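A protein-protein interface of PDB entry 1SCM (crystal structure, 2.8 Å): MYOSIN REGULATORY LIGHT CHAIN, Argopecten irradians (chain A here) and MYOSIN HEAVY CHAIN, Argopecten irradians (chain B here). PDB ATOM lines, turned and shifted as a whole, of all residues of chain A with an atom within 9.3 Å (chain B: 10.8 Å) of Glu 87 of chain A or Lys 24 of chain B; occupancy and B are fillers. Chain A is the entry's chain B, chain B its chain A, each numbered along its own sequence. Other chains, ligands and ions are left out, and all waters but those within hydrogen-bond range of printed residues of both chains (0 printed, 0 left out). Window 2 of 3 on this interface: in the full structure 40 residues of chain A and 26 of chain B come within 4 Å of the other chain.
Of the printed residues of chain B, Ala 81 of chain A touches Gly 31.
Glu 87 of chain A touches one residue of chain B.
No residue of chain B comes within 4 Å of Gln 88 of chain A.
Of chain A, only Met 84 and Glu 87 come within 4 Å of Lys 24 of chain B.
Of the printed residues of chain A, Gly 31 of chain B touches Ala 81 and Met 84.
Of the printed residues of chain A, Leu 32 of chain B touches Phe 85.
The nearest residue of chain B that does not touch Glu 87 of chain A is Gln 28 of chain B (4.2 Å).
Of the 17 printed residues of chain A, 4 touch a printed residue of chain B.
Hydrophobic or aromatic side chains of chain A that line the printed part of chain B: Ala 81, Met 84 and Phe 85.
Among the printed residues, 8 pairs touch across the chains.
Among the printed residues, Asp or Glu carboxylates within 4 Å of a Lys or Arg side-chain nitrogen of the other chain: Glu 87 of chain A with Lys 24 of chain B (3.7 Å).
The side-chain sulfur (SD) of Met 84 of chain A lies close to the backbone carbonyl oxygen (O) of Asp 27 of chain B (3.6 Å).
O of Met 84 of chain A lies within hydrogen-bond range of NE2 of Gln 28 of chain B (3.4 Å).
The backbone NH (N) of Gly 31 of chain B sits close to the side-chain sulfur (SD) of Met 84 of chain A.
O of Ala 81 of chain A lies close to O of Gly 31 of chain B (3.4 Å).
NZ of Lys 24 of chain B lies within salt-bridge range of OE1 of Glu 87 of chain A (3.7 Å).
Lys 24 of chain B touches Met 84 of chain A (NZ to O, 3.6 Å).
Gln 28 of chain B touches Phe 85 of chain A (O to CZ, 3.5 Å).
Leu 32 of chain B touches Phe 85 of chain A (N to CZ, 3.99 Å).
The backbone carbonyl oxygen (O) of Lys 24 of chain B sits close to the side-chain amide oxygen (OE1) of Gln 28 of chain B (2.9 Å).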
ATOM      1  N   ASN A  80      11.221  -4.044  24.915  1.00  0.00           N
ATOM      2  CA  ASN A  80      10.351  -3.020  25.414  1.00  0.00           C
ATOM      3  C   ASN A  80      11.005  -1.753  24.857  1.00  0.00           C
ATOM      4  O   ASN A  80      10.304  -0.802  24.484  1.00  0.00           O
ATOM      5  CB  ASN A  80      10.349  -2.919  26.958  1.00  0.00           C
ATOM      6  CG  ASN A  80       9.869  -4.073  27.848  1.00  0.00           C
ATOM      7  OD1 ASN A  80       9.958  -3.960  29.079  1.00  0.00           O
ATOM      8  ND2 ASN A  80       9.392  -5.210  27.324  1.00  0.00           N
ATOM      9  N   ALA A  81      12.356  -1.784  24.745  1.00  0.00           N
ATOM     10  CA  ALA A  81      13.130  -0.672  24.217  1.00  0.00           C
ATOM     11  C   ALA A  81      13.102  -0.474  22.715  1.00  0.00           C
ATOM     12  O   ALA A  81      13.671   0.493  22.208  1.00  0.00           O
ATOM     13  CB  ALA A  81      14.572  -0.812  24.599  1.00  0.00           C
ATOM     14  N   PHE A  82      12.489  -1.404  21.975  1.00  0.00           N
ATOM     15  CA  PHE A  82      12.333  -1.286  20.534  1.00  0.00           C
ATOM     16  C   PHE A  82      10.858  -1.037  20.262  1.00  0.00           C
ATOM     17  O   PHE A  82      10.466  -0.370  19.305  1.00  0.00           O
ATOM     18  CB  PHE A  82      12.714  -2.555  19.841  1.00  0.00           C
ATOM     19  CG  PHE A  82      14.157  -2.901  19.477  1.00  0.00           C
ATOM     20  CD1 PHE A  82      14.757  -2.337  18.359  1.00  0.00           C
ATOM     21  CD2 PHE A  82      14.846  -3.861  20.218  1.00  0.00           C
ATOM     22  CE1 PHE A  82      16.034  -2.741  17.988  1.00  0.00           C
ATOM     23  CE2 PHE A  82      16.122  -4.256  19.832  1.00  0.00           C
ATOM     24  CZ  PHE A  82      16.719  -3.701  18.718  1.00  0.00           C
ATOM     25  N   ALA A  83       9.985  -1.573  21.108  1.00  0.00           N
ATOM     26  CA  ALA A  83       8.550  -1.365  20.991  1.00  0.00           C
ATOM     27  C   ALA A  83       8.133   0.099  21.177  1.00  0.00           C
ATOM     28  O   ALA A  83       7.074   0.534  20.745  1.00  0.00           O
ATOM     29  CB  ALA A  83       7.880  -2.256  22.020  1.00  0.00           C
ATOM     30  N   MET A  84       8.987   0.914  21.798  1.00  0.00           N
ATOM     31  CA  MET A  84       8.800   2.354  21.960  1.00  0.00           C
ATOM     32  C   MET A  84       8.640   3.061  20.609  1.00  0.00           C
ATOM     33  O   MET A  84       8.016   4.130  20.504  1.00  0.00           O
ATOM     34  CB  MET A  84      10.027   2.930  22.726  1.00  0.00           C
ATOM     35  CG  MET A  84       9.861   3.120  24.232  1.00  0.00           C
ATOM     36  SD  MET A  84      11.446   3.357  25.091  1.00  0.00           S
ATOM     37  CE  MET A  84      11.014   2.936  26.750  1.00  0.00           C
ATOM     38  N   PHE A  85       9.243   2.436  19.584  1.00  0.00           N
ATOM     39  CA  PHE A  85       9.296   2.945  18.237  1.00  0.00           C
ATOM     40  C   PHE A  85       8.248   2.248  17.425  1.00  0.00           C
ATOM     41  O   PHE A  85       7.925   2.692  16.341  1.00  0.00           O
ATOM     42  CB  PHE A  85      10.691   2.681  17.692  1.00  0.00           C
ATOM     43  CG  PHE A  85      11.753   3.296  18.598  1.00  0.00           C
ATOM     44  CD1 PHE A  85      12.059   4.663  18.494  1.00  0.00           C
ATOM     45  CD2 PHE A  85      12.345   2.543  19.597  1.00  0.00           C
ATOM     46  CE1 PHE A  85      12.935   5.286  19.386  1.00  0.00           C
ATOM     47  CE2 PHE A  85      13.209   3.155  20.489  1.00  0.00           C
ATOM     48  CZ  PHE A  85      13.502   4.519  20.386  1.00  0.00           C
ATOM     49  N   ASP A  86       7.717   1.155  17.951  1.00  0.00           N
ATOM     50  CA  ASP A  86       6.724   0.306  17.307  1.00  0.00           C
ATOM     51  C   ASP A  86       5.397   0.571  18.023  1.00  0.00           C
ATOM     52  O   ASP A  86       4.959  -0.234  18.844  1.00  0.00           O
ATOM     53  CB  ASP A  86       7.199  -1.167  17.459  1.00  0.00           C
ATOM     54  CG  ASP A  86       6.224  -2.208  16.946  1.00  0.00           C
ATOM     55  OD1 ASP A  86       5.639  -1.980  15.885  1.00  0.00           O
ATOM     56  OD2 ASP A  86       6.035  -3.227  17.614  1.00  0.00           O
ATOM     57  N   GLU A  87       4.687   1.660  17.694  1.00  0.00           N
ATOM     58  CA  GLU A  87       3.539   2.093  18.483  1.00  0.00           C
ATOM     59  C   GLU A  87       2.325   1.156  18.395  1.00  0.00           C
ATOM     60  O   GLU A  87       1.618   0.983  19.384  1.00  0.00           O
ATOM     61  CB  GLU A  87       3.123   3.542  18.064  1.00  0.00           C
ATOM     62  CG  GLU A  87       4.164   4.611  17.579  1.00  0.00           C
ATOM     63  CD  GLU A  87       5.250   5.224  18.496  1.00  0.00           C
ATOM     64  OE1 GLU A  87       5.117   5.194  19.730  1.00  0.00           O
ATOM     65  OE2 GLU A  87       6.235   5.761  17.953  1.00  0.00           O
ATOM     66  N   GLN A  88       2.107   0.468  17.259  1.00  0.00           N
ATOM     67  CA  GLN A  88       0.948  -0.405  16.991  1.00  0.00           C
ATOM     68  C   GLN A  88       1.141  -1.861  17.406  1.00  0.00           C
ATOM     69  O   GLN A  88       0.308  -2.710  17.101  1.00  0.00           O
ATOM     70  CB  GLN A  88       0.639  -0.345  15.476  1.00  0.00           C
ATOM     71  CG  GLN A  88      -0.817  -0.439  14.935  1.00  0.00           C
ATOM     72  CD  GLN A  88      -1.524   0.862  14.494  1.00  0.00           C
ATOM     73  OE1 GLN A  88      -0.934   1.873  14.104  1.00  0.00           O
ATOM     74  NE2 GLN A  88      -2.850   0.859  14.512  1.00  0.00           N
ATOM     75  N   GLU A  89       2.222  -2.180  18.107  1.00  0.00           N
ATOM     76  CA  GLU A  89       2.614  -3.527  18.457  1.00  0.00           C
ATOM     77  C   GLU A  89       2.845  -4.497  17.297  1.00  0.00           C
ATOM     78  O   GLU A  89       2.697  -5.694  17.504  1.00  0.00           O
ATOM     79  CB  GLU A  89       1.579  -4.091  19.426  1.00  0.00           C
ATOM     80  CG  GLU A  89       1.890  -3.689  20.859  1.00  0.00           C
ATOM     81  CD  GLU A  89       0.695  -3.773  21.815  1.00  0.00           C
ATOM     82  OE1 GLU A  89       0.151  -4.872  21.979  1.00  0.00           O
ATOM     83  OE2 GLU A  89       0.308  -2.745  22.392  1.00  0.00           O
ATOM     84  N   THR A  90       3.220  -4.095  16.066  1.00  0.00           N
ATOM     85  CA  THR A  90       3.509  -5.036  14.964  1.00  0.00           C
ATOM     86  C   THR A  90       4.881  -5.519  15.342  1.00  0.00           C
ATOM     87  O   THR A  90       5.768  -4.694  15.237  1.00  0.00           O
ATOM     88  CB  THR A  90       3.565  -4.318  13.609  1.00  0.00           C
ATOM     89  OG1 THR A  90       4.241  -3.085  13.775  1.00  0.00           O
ATOM     90  CG2 THR A  90       2.193  -3.966  13.097  1.00  0.00           C
ATOM     91  N   LYS A  91       5.196  -6.730  15.783  1.00  0.00           N
ATOM     92  CA  LYS A  91       6.518  -6.946  16.376  1.00  0.00           C
ATOM     93  C   LYS A  91       7.708  -7.108  15.426  1.00  0.00           C
ATOM     94  O   LYS A  91       8.478  -8.071  15.407  1.00  0.00           O
ATOM     95  CB  LYS A  91       6.366  -8.134  17.340  1.00  0.00           C
ATOM     96  CG  LYS A  91       5.380  -7.831  18.481  1.00  0.00           C
ATOM     97  CD  LYS A  91       5.659  -8.699  19.707  1.00  0.00           C
ATOM     98  CE  LYS A  91       6.734  -8.091  20.639  1.00  0.00           C
ATOM     99  NZ  LYS A  91       7.525  -9.105  21.328  1.00  0.00           N
ATOM    100  N   LYS A  92       7.919  -5.961  14.792  1.00  0.00           N
ATOM    101  CA  LYS A  92       8.831  -5.670  13.692  1.00  0.00           C
ATOM    102  C   LYS A  92       9.040  -4.155  13.616  1.00  0.00           C
ATOM    103  O   LYS A  92       8.270  -3.382  14.189  1.00  0.00           O
ATOM    104  CB  LYS A  92       8.252  -6.111  12.362  1.00  0.00           C
ATOM    105  CG  LYS A  92       8.418  -7.589  12.279  1.00  0.00           C
ATOM    106  CD  LYS A  92       7.436  -8.201  11.356  1.00  0.00           C
ATOM    107  CE  LYS A  92       7.224  -9.562  11.976  1.00  0.00           C
ATOM    108  NZ  LYS A  92       6.207  -9.410  12.998  1.00  0.00           N
ATOM    109  N   LEU A  93      10.040  -3.658  12.900  1.00  0.00           N
ATOM    110  CA  LEU A  93      10.264  -2.222  12.809  1.00  0.00           C
ATOM    111  C   LEU A  93      10.762  -1.990  11.375  1.00  0.00           C
ATOM    112  O   LEU A  93      11.541  -2.787  10.852  1.00  0.00           O
ATOM    113  CB  LEU A  93      11.290  -1.881  13.887  1.00  0.00           C
ATOM    114  CG  LEU A  93      11.368  -0.530  14.528  1.00  0.00           C
ATOM    115  CD1 LEU A  93      10.111  -0.202  15.294  1.00  0.00           C
ATOM    116  CD2 LEU A  93      12.484  -0.554  15.538  1.00  0.00           C
ATOM    117  N   TYR A  97      13.661   2.870   9.355  1.00  0.00           N
ATOM    118  CA  TYR A  97      13.392   3.619  10.571  1.00  0.00           C
ATOM    119  C   TYR A  97      14.543   3.232  11.461  1.00  0.00           C
ATOM    120  O   TYR A  97      15.368   4.086  11.807  1.00  0.00           O
ATOM    121  CB  TYR A  97      12.099   3.208  11.272  1.00  0.00           C
ATOM    122  CG  TYR A  97      11.703   4.029  12.518  1.00  0.00           C
ATOM    123  CD1 TYR A  97      12.204   5.326  12.715  1.00  0.00           C
ATOM    124  CD2 TYR A  97      10.797   3.498  13.457  1.00  0.00           C
ATOM    125  CE1 TYR A  97      11.803   6.080  13.818  1.00  0.00           C
ATOM    126  CE2 TYR A  97      10.392   4.258  14.564  1.00  0.00           C
ATOM    127  CZ  TYR A  97      10.903   5.542  14.724  1.00  0.00           C
ATOM    128  OH  TYR A  97      10.494   6.346  15.757  1.00  0.00           O
ATOM    129  N   LEU A 101      17.559   5.712  12.987  1.00  0.00           N
ATOM    130  CA  LEU A 101      17.657   5.882  14.402  1.00  0.00           C
ATOM    131  C   LEU A 101      19.061   5.634  14.866  1.00  0.00           C
ATOM    132  O   LEU A 101      19.734   6.492  15.440  1.00  0.00           O
ATOM    133  CB  LEU A 101      16.724   4.904  15.090  1.00  0.00           C
ATOM    134  CG  LEU A 101      15.230   5.160  15.091  1.00  0.00           C
ATOM    135  CD1 LEU A 101      14.494   3.921  15.472  1.00  0.00           C
ATOM    136  CD2 LEU A 101      14.912   6.255  16.083  1.00  0.00           C
ATOM    137  N   TYR A 130      12.597  -7.321  15.374  1.00  0.00           N
ATOM    138  CA  TYR A 130      13.356  -7.047  16.583  1.00  0.00           C
ATOM    139  C   TYR A 130      13.111  -7.996  17.743  1.00  0.00           C
ATOM    140  O   TYR A 130      13.821  -7.925  18.744  1.00  0.00           O
ATOM    141  CB  TYR A 130      13.099  -5.624  17.061  1.00  0.00           C
ATOM    142  CG  TYR A 130      11.724  -5.352  17.632  1.00  0.00           C
ATOM    143  CD1 TYR A 130      11.493  -5.523  18.998  1.00  0.00           C
ATOM    144  CD2 TYR A 130      10.706  -4.911  16.801  1.00  0.00           C
ATOM    145  CE1 TYR A 130      10.245  -5.252  19.547  1.00  0.00           C
ATOM    146  CE2 TYR A 130       9.449  -4.639  17.350  1.00  0.00           C
ATOM    147  CZ  TYR A 130       9.228  -4.808  18.718  1.00  0.00           C
ATOM    148  OH  TYR A 130       7.991  -4.516  19.252  1.00  0.00           O
ATOM    149  N   TYR B  16       1.950  23.641  23.236  1.00  0.00           N
ATOM    150  CA  TYR B  16       1.199  22.479  23.691  1.00  0.00           C
ATOM    151  C   TYR B  16       1.737  21.231  23.012  1.00  0.00           C
ATOM    152  O   TYR B  16       2.071  20.317  23.749  1.00  0.00           O
ATOM    153  CB  TYR B  16      -0.272  22.661  23.342  1.00  0.00           C
ATOM    154  CG  TYR B  16      -1.293  21.682  23.891  1.00  0.00           C
ATOM    155  CD1 TYR B  16      -1.209  20.316  23.655  1.00  0.00           C
ATOM    156  CD2 TYR B  16      -2.362  22.193  24.619  1.00  0.00           C
ATOM    157  CE1 TYR B  16      -2.195  19.472  24.146  1.00  0.00           C
ATOM    158  CE2 TYR B  16      -3.355  21.350  25.114  1.00  0.00           C
ATOM    159  CZ  TYR B  16      -3.255  19.996  24.876  1.00  0.00           C
ATOM    160  OH  TYR B  16      -4.177  19.154  25.446  1.00  0.00           O
ATOM    161  N   LEU B  17       1.906  21.140  21.680  1.00  0.00           N
ATOM    162  CA  LEU B  17       2.332  19.909  21.067  1.00  0.00           C
ATOM    163  C   LEU B  17       3.767  19.456  21.334  1.00  0.00           C
ATOM    164  O   LEU B  17       4.014  18.266  21.159  1.00  0.00           O
ATOM    165  CB  LEU B  17       2.065  20.050  19.573  1.00  0.00           C
ATOM    166  CG  LEU B  17       0.674  20.546  19.051  1.00  0.00           C
ATOM    167  CD1 LEU B  17       0.551  20.418  17.561  1.00  0.00           C
ATOM    168  CD2 LEU B  17      -0.417  19.648  19.531  1.00  0.00           C
ATOM    169  N   ILE B  18       4.701  20.322  21.812  1.00  0.00           N
ATOM    170  CA  ILE B  18       6.133  20.058  22.165  1.00  0.00           C
ATOM    171  C   ILE B  18       6.312  19.524  23.564  1.00  0.00           C
ATOM    172  O   ILE B  18       7.192  18.706  23.833  1.00  0.00           O
ATOM    173  CB  ILE B  18       7.049  21.315  22.126  1.00  0.00           C
ATOM    174  CG1 ILE B  18       7.034  21.850  20.716  1.00  0.00           C
ATOM    175  CG2 ILE B  18       8.500  21.020  22.521  1.00  0.00           C
ATOM    176  CD1 ILE B  18       7.652  20.964  19.618  1.00  0.00           C
ATOM    177  N   ARG B  19       5.519  20.041  24.487  1.00  0.00           N
ATOM    178  CA  ARG B  19       5.557  19.538  25.845  1.00  0.00           C
ATOM    179  C   ARG B  19       4.918  18.152  25.943  1.00  0.00           C
ATOM    180  O   ARG B  19       5.208  17.323  26.809  1.00  0.00           O
ATOM    181  CB  ARG B  19       4.841  20.526  26.715  1.00  0.00           C
ATOM    182  CG  ARG B  19       5.440  21.917  26.754  1.00  0.00           C
ATOM    183  CD  ARG B  19       4.773  22.739  27.839  1.00  0.00           C
ATOM    184  NE  ARG B  19       5.231  24.087  27.649  1.00  0.00           N
ATOM    185  CZ  ARG B  19       4.560  24.979  26.918  1.00  0.00           C
ATOM    186  NH1 ARG B  19       3.415  24.700  26.320  1.00  0.00           N
ATOM    187  NH2 ARG B  19       5.095  26.178  26.743  1.00  0.00           N
ATOM    188  N   LYS B  20       4.025  17.918  24.986  1.00  0.00           N
ATOM    189  CA  LYS B  20       3.368  16.648  24.801  1.00  0.00           C
ATOM    190  C   LYS B  20       4.437  15.675  24.305  1.00  0.00           C
ATOM    191  O   LYS B  20       4.782  14.729  25.008  1.00  0.00           O
ATOM    192  CB  LYS B  20       2.232  16.871  23.797  1.00  0.00           C
ATOM    193  CG  LYS B  20       1.411  15.631  23.501  1.00  0.00           C
ATOM    194  CD  LYS B  20       0.846  15.056  24.788  1.00  0.00           C
ATOM    195  CE  LYS B  20       0.147  13.706  24.614  1.00  0.00           C
ATOM    196  NZ  LYS B  20      -0.267  13.176  25.906  1.00  0.00           N
ATOM    197  N   ALA B  21       5.051  15.933  23.136  1.00  0.00           N
ATOM    198  CA  ALA B  21       6.089  15.085  22.576  1.00  0.00           C
ATOM    199  C   ALA B  21       7.286  14.921  23.467  1.00  0.00           C
ATOM    200  O   ALA B  21       8.016  13.945  23.265  1.00  0.00           O
ATOM    201  CB  ALA B  21       6.602  15.633  21.254  1.00  0.00           C
ATOM    202  N   TYR B  22       7.430  15.836  24.457  1.00  0.00           N
ATOM    203  CA  TYR B  22       8.549  15.854  25.400  1.00  0.00           C
ATOM    204  C   TYR B  22       8.607  14.569  26.178  1.00  0.00           C
ATOM    205  O   TYR B  22       9.628  13.905  26.314  1.00  0.00           O
ATOM    206  CB  TYR B  22       8.416  17.005  26.420  1.00  0.00           C
ATOM    207  CG  TYR B  22       9.577  17.190  27.425  1.00  0.00           C
ATOM    208  CD1 TYR B  22      10.851  17.532  26.940  1.00  0.00           C
ATOM    209  CD2 TYR B  22       9.383  17.060  28.817  1.00  0.00           C
ATOM    210  CE1 TYR B  22      11.917  17.753  27.813  1.00  0.00           C
ATOM    211  CE2 TYR B  22      10.455  17.281  29.692  1.00  0.00           C
ATOM    212  CZ  TYR B  22      11.708  17.629  29.171  1.00  0.00           C
ATOM    213  OH  TYR B  22      12.782  17.894  29.981  1.00  0.00           O
ATOM    214  N   LYS B  23       7.422  14.245  26.662  1.00  0.00           N
ATOM    215  CA  LYS B  23       7.200  13.087  27.499  1.00  0.00           C
ATOM    216  C   LYS B  23       7.660  11.848  26.733  1.00  0.00           C
ATOM    217  O   LYS B  23       8.390  11.066  27.325  1.00  0.00           O
ATOM    218  CB  LYS B  23       5.701  13.026  27.824  1.00  0.00           C
ATOM    219  CG  LYS B  23       4.901  14.309  28.194  1.00  0.00           C
ATOM    220  CD  LYS B  23       3.418  14.017  27.852  1.00  0.00           C
ATOM    221  CE  LYS B  23       2.417  15.091  28.257  1.00  0.00           C
ATOM    222  NZ  LYS B  23       2.210  15.235  29.692  1.00  0.00           N
ATOM    223  N   LYS B  24       7.338  11.706  25.415  1.00  0.00           N
ATOM    224  CA  LYS B  24       7.679  10.543  24.575  1.00  0.00           C
ATOM    225  C   LYS B  24       9.065  10.661  23.916  1.00  0.00           C
ATOM    226  O   LYS B  24       9.539   9.739  23.273  1.00  0.00           O
ATOM    227  CB  LYS B  24       6.572  10.377  23.513  1.00  0.00           C
ATOM    228  CG  LYS B  24       6.521   9.223  22.450  1.00  0.00           C
ATOM    229  CD  LYS B  24       5.850   7.809  22.689  1.00  0.00           C
ATOM    230  CE  LYS B  24       6.747   6.706  23.330  1.00  0.00           C
ATOM    231  NZ  LYS B  24       6.188   5.357  23.315  1.00  0.00           N
ATOM    232  N   LEU B  25       9.780  11.774  24.040  1.00  0.00           N
ATOM    233  CA  LEU B  25      11.155  11.931  23.589  1.00  0.00           C
ATOM    234  C   LEU B  25      12.185  11.580  24.670  1.00  0.00           C
ATOM    235  O   LEU B  25      13.384  11.325  24.490  1.00  0.00           O
ATOM    236  CB  LEU B  25      11.345  13.347  23.199  1.00  0.00           C
ATOM    237  CG  LEU B  25      11.591  13.702  21.769  1.00  0.00           C
ATOM    238  CD1 LEU B  25      10.581  13.024  20.899  1.00  0.00           C
ATOM    239  CD2 LEU B  25      11.563  15.221  21.648  1.00  0.00           C
ATOM    240  N   GLN B  26      11.634  11.617  25.864  1.00  0.00           N
ATOM    241  CA  GLN B  26      12.355  11.409  27.093  1.00  0.00           C
ATOM    242  C   GLN B  26      12.613   9.930  27.291  1.00  0.00           C
ATOM    243  O   GLN B  26      13.621   9.545  27.866  1.00  0.00           O
ATOM    244  CB  GLN B  26      11.486  11.971  28.183  1.00  0.00           C
ATOM    245  CG  GLN B  26      12.161  12.272  29.483  1.00  0.00           C
ATOM    246  CD  GLN B  26      12.028  13.755  29.708  1.00  0.00           C
ATOM    247  OE1 GLN B  26      11.262  14.222  30.544  1.00  0.00           O
ATOM    248  NE2 GLN B  26      12.744  14.539  28.915  1.00  0.00           N
ATOM    249  N   ASP B  27      11.637   9.129  26.855  1.00  0.00           N
ATOM    250  CA  ASP B  27      11.664   7.689  26.983  1.00  0.00           C
ATOM    251  C   ASP B  27      12.407   7.097  25.828  1.00  0.00           C
ATOM    252  O   ASP B  27      13.285   6.266  25.994  1.00  0.00           O
ATOM    253  CB  ASP B  27      10.287   7.106  26.962  1.00  0.00           C
ATOM    254  CG  ASP B  27       9.388   7.726  27.999  1.00  0.00           C
ATOM    255  OD1 ASP B  27       9.743   7.707  29.178  1.00  0.00           O
ATOM    256  OD2 ASP B  27       8.333   8.226  27.611  1.00  0.00           O
ATOM    257  N   GLN B  28      12.066   7.549  24.636  1.00  0.00           N
ATOM    258  CA  GLN B  28      12.727   7.063  23.459  1.00  0.00           C
ATOM    259  C   GLN B  28      14.203   7.272  23.521  1.00  0.00           C
ATOM    260  O   GLN B  28      14.890   6.527  22.851  1.00  0.00           O
ATOM    261  CB  GLN B  28      12.175   7.753  22.255  1.00  0.00           C
ATOM    262  CG  GLN B  28      10.725   7.398  22.075  1.00  0.00           C
ATOM    263  CD  GLN B  28      10.195   7.987  20.809  1.00  0.00           C
ATOM    264  OE1 GLN B  28      10.330   9.183  20.500  1.00  0.00           O
ATOM    265  NE2 GLN B  28       9.569   7.070  20.066  1.00  0.00           N
ATOM    266  N   ARG B  29      14.716   8.227  24.317  1.00  0.00           N
ATOM    267  CA  ARG B  29      16.163   8.342  24.573  1.00  0.00           C
ATOM    268  C   ARG B  29      16.681   7.148  25.337  1.00  0.00           C
ATOM    269  O   ARG B  29      17.728   6.605  25.045  1.00  0.00           O
ATOM    270  CB  ARG B  29      16.503   9.582  25.381  1.00  0.00           C
ATOM    271  CG  ARG B  29      17.943   9.624  25.854  1.00  0.00           C
ATOM    272  CD  ARG B  29      18.469  10.989  26.312  1.00  0.00           C
ATOM    273  NE  ARG B  29      17.642  11.722  27.260  1.00  0.00           N
ATOM    274  CZ  ARG B  29      18.141  12.741  27.966  1.00  0.00           C
ATOM    275  NH1 ARG B  29      19.418  13.098  27.843  1.00  0.00           N
ATOM    276  NH2 ARG B  29      17.332  13.467  28.740  1.00  0.00           N
ATOM    277  N   ILE B  30      15.930   6.693  26.304  1.00  0.00           N
ATOM    278  CA  ILE B  30      16.349   5.541  27.060  1.00  0.00           C
ATOM    279  C   ILE B  30      16.199   4.276  26.224  1.00  0.00           C
ATOM    280  O   ILE B  30      17.082   3.421  26.199  1.00  0.00           O
ATOM    281  CB  ILE B  30      15.514   5.584  28.333  1.00  0.00           C
ATOM    282  CG1 ILE B  30      16.068   6.713  29.226  1.00  0.00           C
ATOM    283  CG2 ILE B  30      15.556   4.241  29.020  1.00  0.00           C
ATOM    284  CD1 ILE B  30      15.307   7.186  30.483  1.00  0.00           C
ATOM    285  N   GLY B  31      15.116   4.176  25.470  1.00  0.00           N
ATOM    286  CA  GLY B  31      14.933   3.060  24.589  1.00  0.00           C
ATOM    287  C   GLY B  31      16.037   3.068  23.561  1.00  0.00           C
ATOM    288  O   GLY B  31      16.556   1.989  23.329  1.00  0.00           O
ATOM    289  N   LEU B  32      16.473   4.234  23.033  1.00  0.00           N
ATOM    290  CA  LEU B  32      17.454   4.256  21.949  1.00  0.00           C
ATOM    291  C   LEU B  32      18.817   4.021  22.516  1.00  0.00           C
ATOM    292  O   LEU B  32      19.670   3.426  21.865  1.00  0.00           O
ATOM    293  CB  LEU B  32      17.545   5.573  21.195  1.00  0.00           C
ATOM    294  CG  LEU B  32      18.531   5.678  20.022  1.00  0.00           C
ATOM    295  CD1 LEU B  32      18.156   4.713  18.947  1.00  0.00           C
ATOM    296  CD2 LEU B  32      18.424   6.992  19.323  1.00  0.00           C
